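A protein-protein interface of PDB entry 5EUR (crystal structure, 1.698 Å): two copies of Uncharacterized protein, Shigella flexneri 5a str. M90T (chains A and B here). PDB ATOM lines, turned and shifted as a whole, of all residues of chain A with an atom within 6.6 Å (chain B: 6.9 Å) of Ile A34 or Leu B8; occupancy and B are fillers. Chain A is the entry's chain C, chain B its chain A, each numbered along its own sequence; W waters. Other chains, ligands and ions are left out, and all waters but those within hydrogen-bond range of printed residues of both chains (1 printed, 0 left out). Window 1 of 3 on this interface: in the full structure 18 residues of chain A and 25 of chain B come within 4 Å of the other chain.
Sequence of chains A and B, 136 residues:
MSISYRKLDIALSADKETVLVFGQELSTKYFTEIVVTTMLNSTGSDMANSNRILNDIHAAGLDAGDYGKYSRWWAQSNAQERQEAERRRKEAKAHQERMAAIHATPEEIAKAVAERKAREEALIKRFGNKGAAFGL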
ATOM      1  N   LYS A  29      11.852  12.732  19.870  1.00  0.00           N
ATOM      2  CA  LYS A  29      11.068  12.412  18.682  1.00  0.00           C
ATOM      3  C   LYS A  29      11.726  11.312  17.857  1.00  0.00           C
ATOM      4  O   LYS A  29      11.030  10.467  17.297  1.00  0.00           O
ATOM      5  CB  LYS A  29      10.858  13.658  17.821  1.00  0.00           C
ATOM      6  CG  LYS A  29       9.905  14.661  18.452  1.00  0.00           C
ATOM      7  CD  LYS A  29       9.569  15.780  17.471  1.00  0.00           C
ATOM      8  CE  LYS A  29       9.005  15.221  16.171  1.00  0.00           C
ATOM      9  NZ  LYS A  29       8.236  16.240  15.404  1.00  0.00           N
ATOM     10  N   TYR A  30      13.054  11.292  17.776  1.00  0.00           N
ATOM     11  CA  TYR A  30      13.692  10.183  17.072  1.00  0.00           C
ATOM     12  C   TYR A  30      13.390   8.866  17.773  1.00  0.00           C
ATOM     13  O   TYR A  30      13.001   7.876  17.134  1.00  0.00           O
ATOM     14  CB  TYR A  30      15.204  10.413  16.961  1.00  0.00           C
ATOM     15  CG  TYR A  30      15.926   9.250  16.323  1.00  0.00           C
ATOM     16  CD1 TYR A  30      15.919   9.083  14.941  1.00  0.00           C
ATOM     17  CD2 TYR A  30      16.600   8.316  17.099  1.00  0.00           C
ATOM     18  CE1 TYR A  30      16.562   7.999  14.357  1.00  0.00           C
ATOM     19  CE2 TYR A  30      17.249   7.231  16.521  1.00  0.00           C
ATOM     20  CZ  TYR A  30      17.220   7.080  15.153  1.00  0.00           C
ATOM     21  OH  TYR A  30      17.855   6.003  14.584  1.00  0.00           O
ATOM     22  N   PHE A  31      13.503   8.850  19.099  1.00  0.00           N
ATOM     23  CA  PHE A  31      13.247   7.621  19.838  1.00  0.00           C
ATOM     24  C   PHE A  31      11.808   7.151  19.651  1.00  0.00           C
ATOM     25  O   PHE A  31      11.564   5.973  19.368  1.00  0.00           O
ATOM     26  CB  PHE A  31      13.563   7.821  21.321  1.00  0.00           C
ATOM     27  CG  PHE A  31      13.373   6.589  22.133  1.00  0.00           C
ATOM     28  CD1 PHE A  31      14.211   5.487  21.942  1.00  0.00           C
ATOM     29  CD2 PHE A  31      12.365   6.510  23.079  1.00  0.00           C
ATOM     30  CE1 PHE A  31      14.051   4.328  22.691  1.00  0.00           C
ATOM     31  CE2 PHE A  31      12.198   5.357  23.840  1.00  0.00           C
ATOM     32  CZ  PHE A  31      13.031   4.260  23.640  1.00  0.00           C
ATOM     33  N   THR A  32      10.836   8.064  19.784  1.00  0.00           N
ATOM     34  CA  THR A  32       9.446   7.623  19.741  1.00  0.00           C
ATOM     35  C   THR A  32       8.947   7.381  18.315  1.00  0.00           C
ATOM     36  O   THR A  32       8.113   6.492  18.113  1.00  0.00           O
ATOM     37  CB  THR A  32       8.545   8.632  20.460  1.00  0.00           C
ATOM     38  OG1 THR A  32       8.592   9.897  19.788  1.00  0.00           O
ATOM     39  CG2 THR A  32       9.021   8.792  21.910  1.00  0.00           C
ATOM     40  N   GLU A  33       9.426   8.140  17.323  1.00  0.00           N
ATOM     41  CA  GLU A  33       8.924   7.984  15.957  1.00  0.00           C
ATOM     42  C   GLU A  33       9.650   6.892  15.186  1.00  0.00           C
ATOM     43  O   GLU A  33       9.025   6.212  14.371  1.00  0.00           O
ATOM     44  CB  GLU A  33       9.022   9.302  15.180  1.00  0.00           C
ATOM     45  CG  GLU A  33       8.229  10.449  15.821  1.00  0.00           C
ATOM     46  CD  GLU A  33       6.739  10.403  15.534  1.00  0.00           C
ATOM     47  OE1 GLU A  33       6.291   9.515  14.786  1.00  0.00           O
ATOM     48  OE2 GLU A  33       6.010  11.245  16.099  1.00  0.00           O
ATOM     49  N   ILE A  34      10.954   6.723  15.406  1.00  0.00           N
ATOM     50  CA  ILE A  34      11.721   5.715  14.673  1.00  0.00           C
ATOM     51  C   ILE A  34      11.999   4.468  15.523  1.00  0.00           C
ATOM     52  O   ILE A  34      11.650   3.341  15.134  1.00  0.00           O
ATOM     53  CB  ILE A  34      13.045   6.308  14.160  1.00  0.00           C
ATOM     54  CG1 ILE A  34      12.782   7.504  13.243  1.00  0.00           C
ATOM     55  CG2 ILE A  34      13.861   5.215  13.467  1.00  0.00           C
ATOM     56  CD1 ILE A  34      12.261   7.138  11.875  1.00  0.00           C
ATOM     57  N   VAL A  35      12.642   4.658  16.683  1.00  0.00           N
ATOM     58  CA  VAL A  35      13.163   3.512  17.428  1.00  0.00           C
ATOM     59  C   VAL A  35      12.029   2.652  17.962  1.00  0.00           C
ATOM     60  O   VAL A  35      11.995   1.439  17.730  1.00  0.00           O
ATOM     61  CB  VAL A  35      14.099   3.968  18.559  1.00  0.00           C
ATOM     62  CG1 VAL A  35      14.658   2.748  19.316  1.00  0.00           C
ATOM     63  CG2 VAL A  35      15.237   4.785  17.961  1.00  0.00           C
ATOM     64  N   VAL A  36      11.094   3.255  18.700  1.00  0.00           N
ATOM     65  CA  VAL A  36      10.043   2.457  19.324  1.00  0.00           C
ATOM     66  C   VAL A  36       9.163   1.801  18.268  1.00  0.00           C
ATOM     67  O   VAL A  36       8.811   0.621  18.385  1.00  0.00           O
ATOM     68  CB  VAL A  36       9.210   3.314  20.299  1.00  0.00           C
ATOM     69  CG1 VAL A  36       8.055   2.488  20.834  1.00  0.00           C
ATOM     70  CG2 VAL A  36      10.102   3.828  21.426  1.00  0.00           C
ATOM     71  N   THR A  37       8.793   2.549  17.224  1.00  0.00           N
ATOM     72  CA  THR A  37       7.991   1.970  16.153  1.00  0.00           C
ATOM     73  C   THR A  37       8.679   0.747  15.563  1.00  0.00           C
ATOM     74  O   THR A  37       8.024  -0.271  15.301  1.00  0.00           O
ATOM     75  CB  THR A  37       7.754   3.016  15.059  1.00  0.00           C
ATOM     76  OG1 THR A  37       7.151   4.185  15.633  1.00  0.00           O
ATOM     77  CG2 THR A  37       6.843   2.455  13.963  1.00  0.00           C
ATOM     78  N   THR A  38      10.003   0.829  15.360  1.00  0.00           N
ATOM     79  CA  THR A  38      10.738  -0.284  14.759  1.00  0.00           C
ATOM     80  C   THR A  38      10.841  -1.468  15.725  1.00  0.00           C
ATOM     81  O   THR A  38      10.672  -2.625  15.321  1.00  0.00           O
ATOM     82  CB  THR A  38      12.131   0.182  14.314  1.00  0.00           C
ATOM     83  OG1 THR A  38      12.007   1.343  13.458  1.00  0.00           O
ATOM     84  CG2 THR A  38      12.822  -0.945  13.525  1.00  0.00           C
ATOM     85  N   MET A  39      11.089  -1.202  17.009  1.00  0.00           N
ATOM     86  CA  MET A  39      11.107  -2.288  17.992  1.00  0.00           C
ATOM     87  C   MET A  39       9.783  -3.048  17.978  1.00  0.00           C
ATOM     88  O   MET A  39       9.746  -4.294  17.936  1.00  0.00           O
ATOM     89  CB  MET A  39      11.367  -1.734  19.401  1.00  0.00           C
ATOM     90  CG  MET A  39      12.772  -1.117  19.628  1.00  0.00           C
ATOM     91  SD  MET A  39      12.808  -0.170  21.170  1.00  0.00           S
ATOM     92  CE  MET A  39      12.542  -1.486  22.351  1.00  0.00           C
ATOM     93  N   TYR B   5       5.128   4.517   9.799  1.00  0.00           N
ATOM     94  CA  TYR B   5       5.854   5.652  10.335  1.00  0.00           C
ATOM     95  C   TYR B   5       5.202   6.934   9.853  1.00  0.00           C
ATOM     96  O   TYR B   5       4.579   6.973   8.788  1.00  0.00           O
ATOM     97  CB  TYR B   5       7.316   5.626   9.870  1.00  0.00           C
ATOM     98  CG  TYR B   5       8.058   4.403  10.328  1.00  0.00           C
ATOM     99  CD1 TYR B   5       8.870   4.449  11.459  1.00  0.00           C
ATOM    100  CD2 TYR B   5       7.947   3.194   9.645  1.00  0.00           C
ATOM    101  CE1 TYR B   5       9.532   3.334  11.899  1.00  0.00           C
ATOM    102  CE2 TYR B   5       8.604   2.075  10.083  1.00  0.00           C
ATOM    103  CZ  TYR B   5       9.398   2.149  11.203  1.00  0.00           C
ATOM    104  OH  TYR B   5      10.063   1.043  11.649  1.00  0.00           O
ATOM    105  N   ARG B   6       5.341   7.987  10.646  1.00  0.00           N
ATOM    106  CA  ARG B   6       4.966   9.292  10.142  1.00  0.00           C
ATOM    107  C   ARG B   6       5.942   9.686   9.027  1.00  0.00           C
ATOM    108  O   ARG B   6       6.969   9.035   8.807  1.00  0.00           O
ATOM    109  CB  ARG B   6       4.945  10.297  11.294  1.00  0.00           C
ATOM    110  CG  ARG B   6       3.859   9.913  12.306  1.00  0.00           C
ATOM    111  CD  ARG B   6       3.615  10.901  13.434  1.00  0.00           C
ATOM    112  NE  ARG B   6       2.590  10.344  14.320  1.00  0.00           N
ATOM    113  CZ  ARG B   6       1.279  10.499  14.176  1.00  0.00           C
ATOM    114  NH1 ARG B   6       0.788  11.261  13.204  1.00  0.00           N
ATOM    115  NH2 ARG B   6       0.460   9.913  15.039  1.00  0.00           N
ATOM    116  N   LYS B   7       5.589  10.725   8.275  1.00  0.00           N
ATOM    117  CA  LYS B   7       6.492  11.251   7.261  1.00  0.00           C
ATOM    118  C   LYS B   7       7.867  11.507   7.856  1.00  0.00           C
ATOM    119  O   LYS B   7       7.995  12.233   8.847  1.00  0.00           O
ATOM    120  CB  LYS B   7       5.919  12.546   6.676  1.00  0.00           C
ATOM    121  CG  LYS B   7       6.861  13.230   5.699  1.00  0.00           C
ATOM    122  CD  LYS B   7       7.572  14.380   6.417  1.00  0.00           C
ATOM    123  CE  LYS B   7       8.672  15.001   5.588  1.00  0.00           C
ATOM    124  NZ  LYS B   7       9.414  16.014   6.376  1.00  0.00           N
ATOM    125  N   LEU B   8       8.893  10.904   7.259  1.00  0.00           N
ATOM    126  CA  LEU B   8      10.213  10.933   7.874  1.00  0.00           C
ATOM    127  C   LEU B   8      10.834  12.306   7.698  1.00  0.00           C
ATOM    128  O   LEU B   8      10.967  12.802   6.574  1.00  0.00           O
ATOM    129  CB  LEU B   8      11.118   9.857   7.281  1.00  0.00           C
ATOM    130  CG  LEU B   8      10.638   8.404   7.384  1.00  0.00           C
ATOM    131  CD1 LEU B   8      11.674   7.485   6.749  1.00  0.00           C
ATOM    132  CD2 LEU B   8      10.376   8.006   8.839  1.00  0.00           C
ATOM    133  N   ASP B   9      11.211  12.908   8.817  1.00  0.00           N
ATOM    134  CA  ASP B   9      11.845  14.218   8.859  1.00  0.00           C
ATOM    135  C   ASP B   9      13.339  13.980   8.731  1.00  0.00           C
ATOM    136  O   ASP B   9      14.035  13.780   9.727  1.00  0.00           O
ATOM    137  CB  ASP B   9      11.494  14.923  10.164  1.00  0.00           C
ATOM    138  CG  ASP B   9      12.196  16.250  10.320  1.00  0.00           C
ATOM    139  OD1 ASP B   9      12.654  16.811   9.301  1.00  0.00           O
ATOM    140  OD2 ASP B   9      12.298  16.725  11.469  1.00  0.00           O
ATOM    141  N   ILE B  10      13.835  13.986   7.490  1.00  0.00           N
ATOM    142  CA  ILE B  10      15.236  13.695   7.199  1.00  0.00           C
ATOM    143  C   ILE B  10      15.844  14.852   6.418  1.00  0.00           C
ATOM    144  O   ILE B  10      15.349  15.215   5.343  1.00  0.00           O
ATOM    145  CB  ILE B  10      15.413  12.399   6.387  1.00  0.00           C
ATOM    146  CG1 ILE B  10      14.742  11.201   7.054  1.00  0.00           C
ATOM    147  CG2 ILE B  10      16.885  12.108   6.194  1.00  0.00           C
ATOM    148  CD1 ILE B  10      14.620  10.021   6.079  1.00  0.00           C
ATOM    149  N   ALA B  11      16.956  15.376   6.917  1.00  0.00           N
ATOM    150  CA  ALA B  11      17.746  16.355   6.183  1.00  0.00           C
ATOM    151  C   ALA B  11      19.168  15.843   6.074  1.00  0.00           C
ATOM    152  O   ALA B  11      19.751  15.416   7.074  1.00  0.00           O
ATOM    153  CB  ALA B  11      17.724  17.719   6.872  1.00  0.00           C
ATOM    154  N   VAL B  21      17.436  13.462  11.616  1.00  0.00           N
ATOM    155  CA  VAL B  21      16.235  12.640  11.546  1.00  0.00           C
ATOM    156  C   VAL B  21      15.451  12.911  12.821  1.00  0.00           C
ATOM    157  O   VAL B  21      15.894  12.533  13.908  1.00  0.00           O
ATOM    158  CB  VAL B  21      16.569  11.145  11.413  1.00  0.00           C
ATOM    159  CG1 VAL B  21      15.294  10.317  11.169  1.00  0.00           C
ATOM    160  CG2 VAL B  21      17.593  10.910  10.300  1.00  0.00           C
ATOM    161  N   PHE B  22      14.309  13.584  12.700  1.00  0.00           N
ATOM    162  CA  PHE B  22      13.474  13.894  13.872  1.00  0.00           C
ATOM    163  C   PHE B  22      14.299  14.521  15.002  1.00  0.00           C
ATOM    164  O   PHE B  22      14.177  14.153  16.170  1.00  0.00           O
ATOM    165  CB  PHE B  22      12.733  12.641  14.357  1.00  0.00           C
ATOM    166  CG  PHE B  22      11.585  12.230  13.464  1.00  0.00           C
ATOM    167  CD1 PHE B  22      10.468  13.039  13.336  1.00  0.00           C
ATOM    168  CD2 PHE B  22      11.618  11.030  12.773  1.00  0.00           C
ATOM    169  CE1 PHE B  22       9.410  12.665  12.522  1.00  0.00           C
ATOM    170  CE2 PHE B  22      10.564  10.647  11.951  1.00  0.00           C
ATOM    171  CZ  PHE B  22       9.462  11.465  11.827  1.00  0.00           C
ATOM    172  N   PHE B  31      22.673   5.575   9.512  1.00  0.00           N
ATOM    173  CA  PHE B  31      21.251   5.651   9.202  1.00  0.00           C
ATOM    174  C   PHE B  31      20.888   4.745   8.026  1.00  0.00           C
ATOM    175  O   PHE B  31      19.902   4.005   8.086  1.00  0.00           O
ATOM    176  CB  PHE B  31      20.855   7.096   8.917  1.00  0.00           C
ATOM    177  CG  PHE B  31      19.398   7.267   8.673  1.00  0.00           C
ATOM    178  CD1 PHE B  31      18.486   7.051   9.703  1.00  0.00           C
ATOM    179  CD2 PHE B  31      18.925   7.639   7.433  1.00  0.00           C
ATOM    180  CE1 PHE B  31      17.126   7.207   9.492  1.00  0.00           C
ATOM    181  CE2 PHE B  31      17.568   7.794   7.220  1.00  0.00           C
ATOM    182  CZ  PHE B  31      16.670   7.580   8.243  1.00  0.00           C
ATOM    183  N   VAL B  35      19.751   1.727  10.295  1.00  0.00           N
ATOM    184  CA  VAL B  35      18.410   2.154  10.694  1.00  0.00           C
ATOM    185  C   VAL B  35      17.383   1.827   9.615  1.00  0.00           C
ATOM    186  O   VAL B  35      16.362   1.186   9.885  1.00  0.00           O
ATOM    187  CB  VAL B  35      18.392   3.644  11.067  1.00  0.00           C
ATOM    188  CG1 VAL B  35      16.983   4.026  11.519  1.00  0.00           C
ATOM    189  CG2 VAL B  35      19.358   3.879  12.202  1.00  0.00           C
ATOM    190  N   VAL B  36      17.623   2.271   8.379  1.00  0.00           N
ATOM    191  CA  VAL B  36      16.619   2.079   7.340  1.00  0.00           C
ATOM    192  C   VAL B  36      16.429   0.602   7.040  1.00  0.00           C
ATOM    193  O   VAL B  36      15.301   0.129   6.887  1.00  0.00           O
ATOM    194  CB  VAL B  36      17.000   2.887   6.084  1.00  0.00           C
ATOM    195  CG1 VAL B  36      16.019   2.597   4.946  1.00  0.00           C
ATOM    196  CG2 VAL B  36      17.029   4.373   6.427  1.00  0.00           C
ATOM    197  N   MET B  39      14.225  -0.754   9.734  1.00  0.00           N
ATOM    198  CA  MET B  39      12.842  -0.292   9.561  1.00  0.00           C
ATOM    199  C   MET B  39      12.126  -1.118   8.501  1.00  0.00           C
ATOM    200  O   MET B  39      10.984  -1.583   8.701  1.00  0.00           O
ATOM    201  CB  MET B  39      12.812   1.189   9.170  1.00  0.00           C
ATOM    202  CG  MET B  39      13.268   2.153  10.289  1.00  0.00           C
ATOM    203  SD  MET B  39      13.566   3.816   9.604  1.00  0.00           S
ATOM    204  CE  MET B  39      11.926   4.260   9.035  1.00  0.00           C
ATOM    205  N   ARG B  52       6.053   3.673   1.555  1.00  0.00           N
ATOM    206  CA  ARG B  52       6.078   4.980   2.215  1.00  0.00           C
ATOM    207  C   ARG B  52       7.480   5.329   2.711  1.00  0.00           C
ATOM    208  O   ARG B  52       7.995   6.437   2.472  1.00  0.00           O
ATOM    209  CB  ARG B  52       5.094   5.004   3.391  1.00  0.00           C
ATOM    210  CG  ARG B  52       3.627   5.182   3.027  1.00  0.00           C
ATOM    211  CD  ARG B  52       2.750   5.162   4.300  1.00  0.00           C
ATOM    212  NE  ARG B  52       3.215   6.125   5.303  1.00  0.00           N
ATOM    213  CZ  ARG B  52       2.754   7.367   5.442  1.00  0.00           C
ATOM    214  NH1 ARG B  52       1.792   7.817   4.649  1.00  0.00           N
ATOM    215  NH2 ARG B  52       3.250   8.161   6.383  1.00  0.00           N
ATOM    216  N   ILE B  53       8.097   4.400   3.448  1.00  0.00           N
ATOM    217  CA  ILE B  53       9.444   4.641   3.958  1.00  0.00           C
ATOM    218  C   ILE B  53      10.382   5.030   2.824  1.00  0.00           C
ATOM    219  O   ILE B  53      11.123   6.017   2.913  1.00  0.00           O
ATOM    220  CB  ILE B  53       9.963   3.397   4.696  1.00  0.00           C
ATOM    221  CG1 ILE B  53       9.159   3.169   5.980  1.00  0.00           C
ATOM    222  CG2 ILE B  53      11.429   3.561   5.019  1.00  0.00           C
ATOM    223  CD1 ILE B  53       9.335   1.748   6.535  1.00  0.00           C
ATOM    224  N   LEU B  54      10.369   4.250   1.739  1.00  0.00           N
ATOM    225  CA  LEU B  54      11.339   4.479   0.668  1.00  0.00           C
ATOM    226  C   LEU B  54      11.032   5.753  -0.108  1.00  0.00           C
ATOM    227  O   LEU B  54      11.953   6.388  -0.628  1.00  0.00           O
ATOM    228  CB  LEU B  54      11.417   3.255  -0.244  1.00  0.00           C
ATOM    229  CG  LEU B  54      12.153   2.087   0.444  1.00  0.00           C
ATOM    230  CD1 LEU B  54      12.089   0.814  -0.380  1.00  0.00           C
ATOM    231  CD2 LEU B  54      13.615   2.468   0.712  1.00  0.00           C
ATOM    232  N   ASP B  56      10.063   8.440   1.407  1.00  0.00           N
ATOM    233  CA  ASP B  56      10.709   9.462   2.235  1.00  0.00           C
ATOM    234  C   ASP B  56      12.233   9.411   2.132  1.00  0.00           C
ATOM    235  O   ASP B  56      12.908  10.458   2.193  1.00  0.00           O
ATOM    236  CB  ASP B  56      10.249   9.305   3.683  1.00  0.00           C
ATOM    237  CG  ASP B  56       8.794   9.679   3.855  1.00  0.00           C
ATOM    238  OD1 ASP B  56       8.236  10.370   2.954  1.00  0.00           O
ATOM    239  OD2 ASP B  56       8.206   9.273   4.867  1.00  0.00           O
ATOM    240  N   ILE B  57      12.793   8.205   1.987  1.00  0.00           N
ATOM    241  CA  ILE B  57      14.230   8.066   1.768  1.00  0.00           C
ATOM    242  C   ILE B  57      14.633   8.764   0.471  1.00  0.00           C
ATOM    243  O   ILE B  57      15.585   9.550   0.439  1.00  0.00           O
ATOM    244  CB  ILE B  57      14.616   6.573   1.759  1.00  0.00           C
ATOM    245  CG1 ILE B  57      14.378   5.951   3.139  1.00  0.00           C
ATOM    246  CG2 ILE B  57      16.049   6.373   1.285  1.00  0.00           C
ATOM    247  CD1 ILE B  57      15.076   6.691   4.278  1.00  0.00           C
ATOM    248  N   ALA B  60      14.474  12.579   0.621  1.00  0.00           N
ATOM    249  CA  ALA B  60      15.543  13.206   1.381  1.00  0.00           C
ATOM    250  C   ALA B  60      16.868  13.268   0.629  1.00  0.00           C
ATOM    251  O   ALA B  60      17.835  13.828   1.157  1.00  0.00           O
ATOM    252  CB  ALA B  60      15.732  12.464   2.708  1.00  0.00           C
ATOM    253  N   ARG B  88      10.072  16.276  -4.291  1.00  0.00           N
ATOM    254  CA  ARG B  88      10.720  16.645  -3.032  1.00  0.00           C
ATOM    255  C   ARG B  88      12.235  16.452  -3.115  1.00  0.00           C
ATOM    256  O   ARG B  88      13.002  17.286  -2.619  1.00  0.00           O
ATOM    257  CB  ARG B  88      10.100  15.817  -1.901  1.00  0.00           C
ATOM    258  CG  ARG B  88       8.601  16.118  -1.701  1.00  0.00           C
ATOM    259  CD  ARG B  88       7.910  15.246  -0.642  1.00  0.00           C
ATOM    260  NE  ARG B  88       8.634  15.097   0.613  1.00  0.00           N
ATOM    261  CZ  ARG B  88       8.681  13.968   1.316  1.00  0.00           C
ATOM    262  NH1 ARG B  88       8.052  12.878   0.884  1.00  0.00           N
ATOM    263  NH2 ARG B  88       9.360  13.928   2.452  1.00  0.00           N
HETATM  264  O   HOH W   1       6.703   7.425  13.199  1.00  0.00           O
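The side-chain hydroxyl (OH) of Tyr B5 sits at hydrogen-bond distance from the side-chain hydroxyl (OG1) of Thr A38, 2.7 Å away. The side-chain carboxylate (OE1) of Glu A33 lies within salt-bridge range of the guanidinium group (NE) of Arg B6, 3.8 Å away. The backbone carbonyl oxygen of Phe B22 lies within hydrogen-bond range of the backbone NH of Tyr A30, 3.5 Å away.
NH2 of Arg B52 sits at hydrogen-bond distance from O of Tyr B5, 3.0 Å away. The side-chain carboxylate (OD2) of Asp B56 sits at hydrogen-bond distance from the backbone NH (N) of Leu B8, 3.0 Å away. The backbone carbonyl oxygen (O) of Asp B9 lies within hydrogen-bond range of the backbone NH (N) of Phe B22 (3.0 Å). The backbone NH (N) of Val A35 is in hydrogen-bond range of the backbone carbonyl oxygen (O) of Tyr A30, 3.3 Å away. The backbone carbonyl oxygen (O) of Glu A33 sits at hydrogen-bond distance from the side-chain hydroxyl (OG1) of Thr A37, 3.0 Å away. The backbone carbonyl oxygen of Ile A34 is in hydrogen-bond range of the side-chain hydroxyl of Thr A38, at 2.6 Å.
Lys A29 touches Phe B22. Tyr A30 touches Val B21 (CD1 to O, 3.6 Å). Tyr A30 touches Val B35 (OH to CG2, 3.5 Å). Tyr B5 touches Glu A33. Glu A33 touches Phe B22 (CB to CE2, 3.8 Å). Tyr B5 touches Ile A34 (CE1 to O, 3.9 Å). Ile A34 touches Leu B8 (CD1 to CD2, 3.7 Å). CG1 of Ile A34 touches CD2 of Phe B22 (3.7 Å). CG2 of Thr A37 touches CE1 of Tyr B5, 3.5 Å away. OG1 of Thr A38 touches CG of Met B39, at 3.5 Å.
Printed residues of chain B within 4 Å of Lys A29: Phe B22 (3.7 Å). Printed residues of chain B within 4 Å of Tyr A30: Val B21, Phe B22 and Val B35. Ile A34 touches just these residues of chain B: Tyr B5, Leu B8, Phe B22 and Val B35. Of the printed residues of chain B, Thr A37 touches Tyr B5 (3.5 Å). Printed residues of chain B within 4 Å of Thr A38: Tyr B5 and Met B39. Leu B8 touches just one residue of chain A: Ile A34 (3.7 Å). Printed residues of chain A within 4 Å of Val B21: Tyr A30. The nearest residue of chain A that does not touch Leu B8 is Glu A33 (6.0 Å).
Of the 11 printed residues of chain A, 6 touch a printed residue of chain B. Printed residues of chain A that touch a printed residue of chain B: Lys A29, Tyr A30, Glu A33, Ile A34, Thr A37 and Thr A38. Along chain A the printed residues that touch a printed residue of chain B span positions 29 to 38. Printed residues of chain B that touch a printed residue of chain A: Tyr B5, Arg B6, Leu B8, Val B21, Phe B22, Val B35 and Met B39. Among the printed residues, 14 pairs touch across the chains. Among the printed residues, Asp or Glu carboxylates within 4 Å of a Lys or Arg side-chain nitrogen of the other chain: Glu A33 with Arg B6 (3.8 Å).
Positions printed for both chains: 31, 35, 36 and 39.
Water W1 bridges OE1 of Glu A33 (2.7 Å) and N of Arg B6 (2.9 Å).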
